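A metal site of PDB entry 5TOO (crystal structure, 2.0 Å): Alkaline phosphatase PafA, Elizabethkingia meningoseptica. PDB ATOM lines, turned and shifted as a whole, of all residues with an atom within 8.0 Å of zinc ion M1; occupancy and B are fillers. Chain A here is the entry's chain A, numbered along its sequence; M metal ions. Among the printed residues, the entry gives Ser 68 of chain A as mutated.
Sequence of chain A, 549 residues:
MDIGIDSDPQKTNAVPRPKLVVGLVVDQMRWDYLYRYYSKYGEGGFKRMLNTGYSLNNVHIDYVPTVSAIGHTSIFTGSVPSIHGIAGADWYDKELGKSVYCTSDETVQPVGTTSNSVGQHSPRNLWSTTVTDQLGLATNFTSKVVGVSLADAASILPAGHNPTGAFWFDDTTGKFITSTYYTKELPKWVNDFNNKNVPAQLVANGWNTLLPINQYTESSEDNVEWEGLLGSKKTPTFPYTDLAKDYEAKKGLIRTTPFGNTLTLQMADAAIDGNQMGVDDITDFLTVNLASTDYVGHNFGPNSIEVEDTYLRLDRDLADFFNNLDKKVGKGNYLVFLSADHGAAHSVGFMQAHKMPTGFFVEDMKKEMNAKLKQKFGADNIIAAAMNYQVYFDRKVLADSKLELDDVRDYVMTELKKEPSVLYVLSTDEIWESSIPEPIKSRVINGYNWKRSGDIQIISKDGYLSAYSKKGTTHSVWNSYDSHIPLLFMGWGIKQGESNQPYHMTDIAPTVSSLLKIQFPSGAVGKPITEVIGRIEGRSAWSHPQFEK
OD1 of Asp 294 touches zinc ion M1, at 3.9 Å.
Four residues have an atom within 4 Å of zinc ion M1: Asp 27, Asp 294, Asp 341 and His 342.
The backbone carbonyl oxygen of Leu 290 sits at hydrogen-bond distance from the backbone NH of Asp 27, 3.1 Å away.
N of Met 29 sits at hydrogen-bond distance from O of His 342 (3.4 Å).
The side-chain amide nitrogen (NE2) of Gln 28 sits at hydrogen-bond distance from the backbone carbonyl oxygen (O) of Asp 294 (3.0 Å).
The side-chain carboxylate of Asp 341 sits at hydrogen-bond distance from the backbone NH of Gln 28, at 3.2 Å.
A ring nitrogen (ND1) of His 475 lies close to a ring nitrogen (ND1) of His 342 (3.3 Å).
N of Asp 294 sits at hydrogen-bond distance from O of Asp 27 (3.4 Å).
ND1 of His 72 lies close to OD2 of Asp 341.
O of Asp 27 lies within hydrogen-bond range of OG1 of Thr 293, at 2.8 Å.
OD1 of Asp 27 binds zinc ion M1.
Zinc ion M1 is bound by NE2 of His 342 (2.1 Å).
The side-chain carboxylate (OD2) of Asp 341 binds zinc ion M1 (2.1 Å).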
ATOM      1  N   VAL A  25      30.128  14.749   6.233  1.00  0.00           N
ATOM      2  CA  VAL A  25      29.793  13.589   5.430  1.00  0.00           C
ATOM      3  C   VAL A  25      28.963  12.664   6.285  1.00  0.00           C
ATOM      4  O   VAL A  25      29.414  12.236   7.356  1.00  0.00           O
ATOM      5  CB  VAL A  25      31.025  12.860   4.880  1.00  0.00           C
ATOM      6  CG1 VAL A  25      30.574  11.697   4.010  1.00  0.00           C
ATOM      7  CG2 VAL A  25      31.927  13.819   4.095  1.00  0.00           C
ATOM      8  N   VAL A  26      27.764  12.361   5.814  1.00  0.00           N
ATOM      9  CA  VAL A  26      26.869  11.429   6.449  1.00  0.00           C
ATOM     10  C   VAL A  26      27.021  10.109   5.717  1.00  0.00           C
ATOM     11  O   VAL A  26      26.594   9.951   4.579  1.00  0.00           O
ATOM     12  CB  VAL A  26      25.416  11.911   6.423  1.00  0.00           C
ATOM     13  CG1 VAL A  26      24.542  10.925   7.229  1.00  0.00           C
ATOM     14  CG2 VAL A  26      25.320  13.349   6.968  1.00  0.00           C
ATOM     15  N   ASP A  27      27.699   9.187   6.370  1.00  0.00           N
ATOM     16  CA  ASP A  27      28.110   7.961   5.737  1.00  0.00           C
ATOM     17  C   ASP A  27      26.905   7.098   5.364  1.00  0.00           C
ATOM     18  O   ASP A  27      25.986   6.904   6.164  1.00  0.00           O
ATOM     19  CB  ASP A  27      29.068   7.229   6.686  1.00  0.00           C
ATOM     20  CG  ASP A  27      30.014   6.337   5.973  1.00  0.00           C
ATOM     21  OD1 ASP A  27      29.555   5.546   5.149  1.00  0.00           O
ATOM     22  OD2 ASP A  27      31.234   6.418   6.265  1.00  0.00           O
ATOM     23  N   GLN A  28      26.873   6.607   4.126  1.00  0.00           N
ATOM     24  CA  GLN A  28      25.780   5.774   3.609  1.00  0.00           C
ATOM     25  C   GLN A  28      24.454   6.525   3.452  1.00  0.00           C
ATOM     26  O   GLN A  28      23.409   5.878   3.211  1.00  0.00           O
ATOM     27  CB  GLN A  28      25.567   4.540   4.492  1.00  0.00           C
ATOM     28  CG  GLN A  28      24.995   3.343   3.766  1.00  0.00           C
ATOM     29  CD  GLN A  28      24.574   2.178   4.715  1.00  0.00           C
ATOM     30  OE1 GLN A  28      23.390   1.884   4.855  1.00  0.00           O
ATOM     31  NE2 GLN A  28      25.565   1.508   5.342  1.00  0.00           N
ATOM     32  N   MET A  29      24.451   7.855   3.523  1.00  0.00           N
ATOM     33  CA  MET A  29      23.214   8.615   3.356  1.00  0.00           C
ATOM     34  C   MET A  29      22.806   8.674   1.883  1.00  0.00           C
ATOM     35  O   MET A  29      23.351   9.449   1.095  1.00  0.00           O
ATOM     36  CB  MET A  29      23.355  10.012   3.920  1.00  0.00           C
ATOM     37  CG  MET A  29      22.065  10.763   3.831  1.00  0.00           C
ATOM     38  SD  MET A  29      22.081  12.379   4.535  1.00  0.00           S
ATOM     39  CE  MET A  29      20.448  12.850   4.004  1.00  0.00           C
ATOM     40  N   THR A  66      31.727   1.831  -5.108  1.00  0.00           N
ATOM     41  CA  THR A  66      31.304   2.845  -4.140  1.00  0.00           C
ATOM     42  C   THR A  66      31.432   2.310  -2.717  1.00  0.00           C
ATOM     43  O   THR A  66      30.454   2.212  -1.949  1.00  0.00           O
ATOM     44  CB  THR A  66      29.870   3.280  -4.438  1.00  0.00           C
ATOM     45  OG1 THR A  66      29.048   2.122  -4.632  1.00  0.00           O
ATOM     46  CG2 THR A  66      29.817   4.167  -5.747  1.00  0.00           C
ATOM     47  N   VAL A  67      32.665   1.972  -2.348  1.00  0.00           N
ATOM     48  CA  VAL A  67      32.936   1.434  -1.019  1.00  0.00           C
ATOM     49  C   VAL A  67      33.471   2.519  -0.085  1.00  0.00           C
ATOM     50  O   VAL A  67      33.541   3.696  -0.423  1.00  0.00           O
ATOM     51  CB  VAL A  67      33.909   0.249  -1.068  1.00  0.00           C
ATOM     52  CG1 VAL A  67      33.288  -0.907  -1.871  1.00  0.00           C
ATOM     53  CG2 VAL A  67      35.247   0.656  -1.680  1.00  0.00           C
ATOM     54  N   SER A  68      33.851   2.070   1.104  1.00  0.00           N
ATOM     55  CA  SER A  68      34.424   2.904   2.129  1.00  0.00           C
ATOM     56  C   SER A  68      35.758   3.507   1.698  1.00  0.00           C
ATOM     57  O   SER A  68      36.427   3.005   0.793  1.00  0.00           O
ATOM     58  CB  SER A  68      34.670   2.047   3.377  1.00  0.00           C
ATOM     59  OG  SER A  68      33.576   1.154   3.541  1.00  0.00           O
ATOM     60  N   ALA A  69      36.142   4.572   2.399  1.00  0.00           N
ATOM     61  CA  ALA A  69      37.418   5.267   2.215  1.00  0.00           C
ATOM     62  C   ALA A  69      37.461   6.076   0.915  1.00  0.00           C
ATOM     63  O   ALA A  69      37.860   7.232   0.941  1.00  0.00           O
ATOM     64  CB  ALA A  69      38.592   4.287   2.258  1.00  0.00           C
ATOM     65  N   ILE A  70      37.030   5.506  -0.203  1.00  0.00           N
ATOM     66  CA  ILE A  70      37.141   6.206  -1.486  1.00  0.00           C
ATOM     67  C   ILE A  70      36.241   7.446  -1.506  1.00  0.00           C
ATOM     68  O   ILE A  70      36.653   8.528  -1.945  1.00  0.00           O
ATOM     69  CB  ILE A  70      36.800   5.285  -2.668  1.00  0.00           C
ATOM     70  CG1 ILE A  70      37.538   3.946  -2.616  1.00  0.00           C
ATOM     71  CG2 ILE A  70      37.102   5.982  -3.989  1.00  0.00           C
ATOM     72  CD1 ILE A  70      37.138   2.969  -3.813  1.00  0.00           C
ATOM     73  N   GLY A  71      34.984   7.286  -1.087  1.00  0.00           N
ATOM     74  CA  GLY A  71      34.063   8.408  -1.121  1.00  0.00           C
ATOM     75  C   GLY A  71      34.571   9.594  -0.327  1.00  0.00           C
ATOM     76  O   GLY A  71      34.501  10.732  -0.777  1.00  0.00           O
ATOM     77  N   HIS A  72      35.071   9.332   0.890  1.00  0.00           N
ATOM     78  CA  HIS A  72      35.666  10.378   1.681  1.00  0.00           C
ATOM     79  C   HIS A  72      36.863  10.977   0.957  1.00  0.00           C
ATOM     80  O   HIS A  72      36.962  12.199   0.802  1.00  0.00           O
ATOM     81  CB  HIS A  72      36.063   9.826   3.072  1.00  0.00           C
ATOM     82  CG  HIS A  72      34.871   9.465   3.902  1.00  0.00           C
ATOM     83  ND1 HIS A  72      34.411   8.178   4.051  1.00  0.00           N
ATOM     84  CD2 HIS A  72      34.009  10.260   4.581  1.00  0.00           C
ATOM     85  CE1 HIS A  72      33.319   8.187   4.797  1.00  0.00           C
ATOM     86  NE2 HIS A  72      33.056   9.441   5.136  1.00  0.00           N
ATOM     87  N   ALA A 154      37.769   7.888   7.718  1.00  0.00           N
ATOM     88  CA  ALA A 154      36.872   9.009   7.504  1.00  0.00           C
ATOM     89  C   ALA A 154      37.292  10.260   8.264  1.00  0.00           C
ATOM     90  O   ALA A 154      36.759  11.347   7.990  1.00  0.00           O
ATOM     91  CB  ALA A 154      35.449   8.568   7.902  1.00  0.00           C
ATOM     92  N   ASN A 289      32.813  13.250   9.734  1.00  0.00           N
ATOM     93  CA  ASN A 289      32.089  12.128   9.161  1.00  0.00           C
ATOM     94  C   ASN A 289      31.177  11.580  10.240  1.00  0.00           C
ATOM     95  O   ASN A 289      31.613  11.345  11.367  1.00  0.00           O
ATOM     96  CB  ASN A 289      33.033  11.029   8.669  1.00  0.00           C
ATOM     97  CG  ASN A 289      32.292   9.741   8.277  1.00  0.00           C
ATOM     98  OD1 ASN A 289      31.463   9.755   7.382  1.00  0.00           O
ATOM     99  ND2 ASN A 289      32.584   8.644   8.955  1.00  0.00           N
ATOM    100  N   LEU A 290      29.906  11.410   9.903  1.00  0.00           N
ATOM    101  CA  LEU A 290      28.909  10.811  10.785  1.00  0.00           C
ATOM    102  C   LEU A 290      28.824   9.341  10.403  1.00  0.00           C
ATOM    103  O   LEU A 290      28.085   8.982   9.481  1.00  0.00           O
ATOM    104  CB  LEU A 290      27.555  11.512  10.651  1.00  0.00           C
ATOM    105  CG  LEU A 290      27.363  12.936  11.206  1.00  0.00           C
ATOM    106  CD1 LEU A 290      27.943  13.112  12.585  1.00  0.00           C
ATOM    107  CD2 LEU A 290      27.917  14.038  10.369  1.00  0.00           C
ATOM    108  N   ALA A 291      29.542   8.485  11.119  1.00  0.00           N
ATOM    109  CA  ALA A 291      29.692   7.092  10.691  1.00  0.00           C
ATOM    110  C   ALA A 291      28.512   6.204  11.055  1.00  0.00           C
ATOM    111  O   ALA A 291      28.360   5.144  10.446  1.00  0.00           O
ATOM    112  CB  ALA A 291      30.958   6.491  11.295  1.00  0.00           C
ATOM    113  N   THR A 293      25.295   6.285  10.718  1.00  0.00           N
ATOM    114  CA  THR A 293      24.318   5.968   9.653  1.00  0.00           C
ATOM    115  C   THR A 293      24.750   4.748   8.852  1.00  0.00           C
ATOM    116  O   THR A 293      23.918   3.968   8.374  1.00  0.00           O
ATOM    117  CB  THR A 293      24.135   7.177   8.726  1.00  0.00           C
ATOM    118  OG1 THR A 293      25.372   7.934   8.655  1.00  0.00           O
ATOM    119  CG2 THR A 293      23.062   8.085   9.254  1.00  0.00           C
ATOM    120  N   ASP A 294      26.055   4.564   8.688  1.00  0.00           N
ATOM    121  CA  ASP A 294      26.557   3.420   7.937  1.00  0.00           C
ATOM    122  C   ASP A 294      26.459   2.134   8.750  1.00  0.00           C
ATOM    123  O   ASP A 294      25.860   1.149   8.295  1.00  0.00           O
ATOM    124  CB  ASP A 294      27.993   3.706   7.511  1.00  0.00           C
ATOM    125  CG  ASP A 294      28.608   2.590   6.740  1.00  0.00           C
ATOM    126  OD1 ASP A 294      28.315   2.443   5.525  1.00  0.00           O
ATOM    127  OD2 ASP A 294      29.403   1.876   7.354  1.00  0.00           O
ATOM    128  N   TYR A 295      27.045   2.130   9.941  1.00  0.00           N
ATOM    129  CA  TYR A 295      26.924   0.976  10.830  1.00  0.00           C
ATOM    130  C   TYR A 295      25.478   0.516  10.979  1.00  0.00           C
ATOM    131  O   TYR A 295      25.170  -0.654  10.792  1.00  0.00           O
ATOM    132  CB  TYR A 295      27.502   1.326  12.198  1.00  0.00           C
ATOM    133  CG  TYR A 295      28.980   1.354  12.162  1.00  0.00           C
ATOM    134  CD1 TYR A 295      29.709   0.181  12.253  1.00  0.00           C
ATOM    135  CD2 TYR A 295      29.655   2.560  12.037  1.00  0.00           C
ATOM    136  CE1 TYR A 295      31.081   0.209  12.243  1.00  0.00           C
ATOM    137  CE2 TYR A 295      31.014   2.609  12.012  1.00  0.00           C
ATOM    138  CZ  TYR A 295      31.734   1.432  12.093  1.00  0.00           C
ATOM    139  OH  TYR A 295      33.112   1.490  12.078  1.00  0.00           O
ATOM    140  N   HIS A 298      24.294  -0.741   7.682  1.00  0.00           N
ATOM    141  CA  HIS A 298      24.830  -2.056   7.343  1.00  0.00           C
ATOM    142  C   HIS A 298      24.077  -3.159   8.063  1.00  0.00           C
ATOM    143  O   HIS A 298      23.937  -4.256   7.517  1.00  0.00           O
ATOM    144  CB  HIS A 298      26.319  -2.142   7.683  1.00  0.00           C
ATOM    145  CG  HIS A 298      27.206  -1.649   6.574  1.00  0.00           C
ATOM    146  ND1 HIS A 298      27.293  -2.294   5.365  1.00  0.00           N
ATOM    147  CD2 HIS A 298      28.009  -0.573   6.494  1.00  0.00           C
ATOM    148  CE1 HIS A 298      28.132  -1.631   4.583  1.00  0.00           C
ATOM    149  NE2 HIS A 298      28.571  -0.579   5.242  1.00  0.00           N
ATOM    150  N   ALA A 340      27.435  12.747   1.183  1.00  0.00           N
ATOM    151  CA  ALA A 340      27.589  11.362   1.575  1.00  0.00           C
ATOM    152  C   ALA A 340      28.701  10.771   0.742  1.00  0.00           C
ATOM    153  O   ALA A 340      28.985  11.248  -0.347  1.00  0.00           O
ATOM    154  CB  ALA A 340      26.320  10.543   1.357  1.00  0.00           C
ATOM    155  N   ASP A 341      29.301   9.689   1.246  1.00  0.00           N
ATOM    156  CA  ASP A 341      30.381   8.998   0.550  1.00  0.00           C
ATOM    157  C   ASP A 341      29.850   7.850  -0.295  1.00  0.00           C
ATOM    158  O   ASP A 341      30.612   7.234  -1.043  1.00  0.00           O
ATOM    159  CB  ASP A 341      31.403   8.504   1.566  1.00  0.00           C
ATOM    160  CG  ASP A 341      30.834   7.463   2.523  1.00  0.00           C
ATOM    161  OD1 ASP A 341      29.623   7.495   2.815  1.00  0.00           O
ATOM    162  OD2 ASP A 341      31.616   6.600   2.969  1.00  0.00           O
ATOM    163  N   HIS A 342      28.554   7.585  -0.195  1.00  0.00           N
ATOM    164  CA  HIS A 342      27.838   6.564  -0.953  1.00  0.00           C
ATOM    165  C   HIS A 342      26.437   6.427  -0.394  1.00  0.00           C
ATOM    166  O   HIS A 342      26.142   6.932   0.698  1.00  0.00           O
ATOM    167  CB  HIS A 342      28.534   5.198  -0.902  1.00  0.00           C
ATOM    168  CG  HIS A 342      28.764   4.688   0.491  1.00  0.00           C
ATOM    169  ND1 HIS A 342      27.783   4.063   1.220  1.00  0.00           N
ATOM    170  CD2 HIS A 342      29.861   4.737   1.291  1.00  0.00           C
ATOM    171  CE1 HIS A 342      28.264   3.737   2.413  1.00  0.00           C
ATOM    172  NE2 HIS A 342      29.521   4.120   2.480  1.00  0.00           N
ATOM    173  N   GLY A 343      25.571   5.761  -1.142  1.00  0.00           N
ATOM    174  CA  GLY A 343      24.232   5.412  -0.713  1.00  0.00           C
ATOM    175  C   GLY A 343      24.219   3.989  -0.182  1.00  0.00           C
ATOM    176  O   GLY A 343      25.156   3.558   0.508  1.00  0.00           O
ATOM    177  N   HIS A 475      26.959  -1.459   0.083  1.00  0.00           N
ATOM    178  CA  HIS A 475      27.143  -0.499  -0.994  1.00  0.00           C
ATOM    179  C   HIS A 475      28.393  -0.894  -1.749  1.00  0.00           C
ATOM    180  O   HIS A 475      29.391  -1.254  -1.123  1.00  0.00           O
ATOM    181  CB  HIS A 475      27.325   0.909  -0.423  1.00  0.00           C
ATOM    182  CG  HIS A 475      28.290   0.960   0.727  1.00  0.00           C
ATOM    183  ND1 HIS A 475      29.607   1.362   0.584  1.00  0.00           N
ATOM    184  CD2 HIS A 475      28.132   0.638   2.033  1.00  0.00           C
ATOM    185  CE1 HIS A 475      30.202   1.307   1.762  1.00  0.00           C
ATOM    186  NE2 HIS A 475      29.334   0.860   2.650  1.00  0.00           N
HETATM  187 ZN    ZN M   1      30.876   4.830   3.853  1.00  0.00          ZN
HETATM  188 ZN    ZN M   2      29.662   1.040   4.750  1.00  0.00          ZN
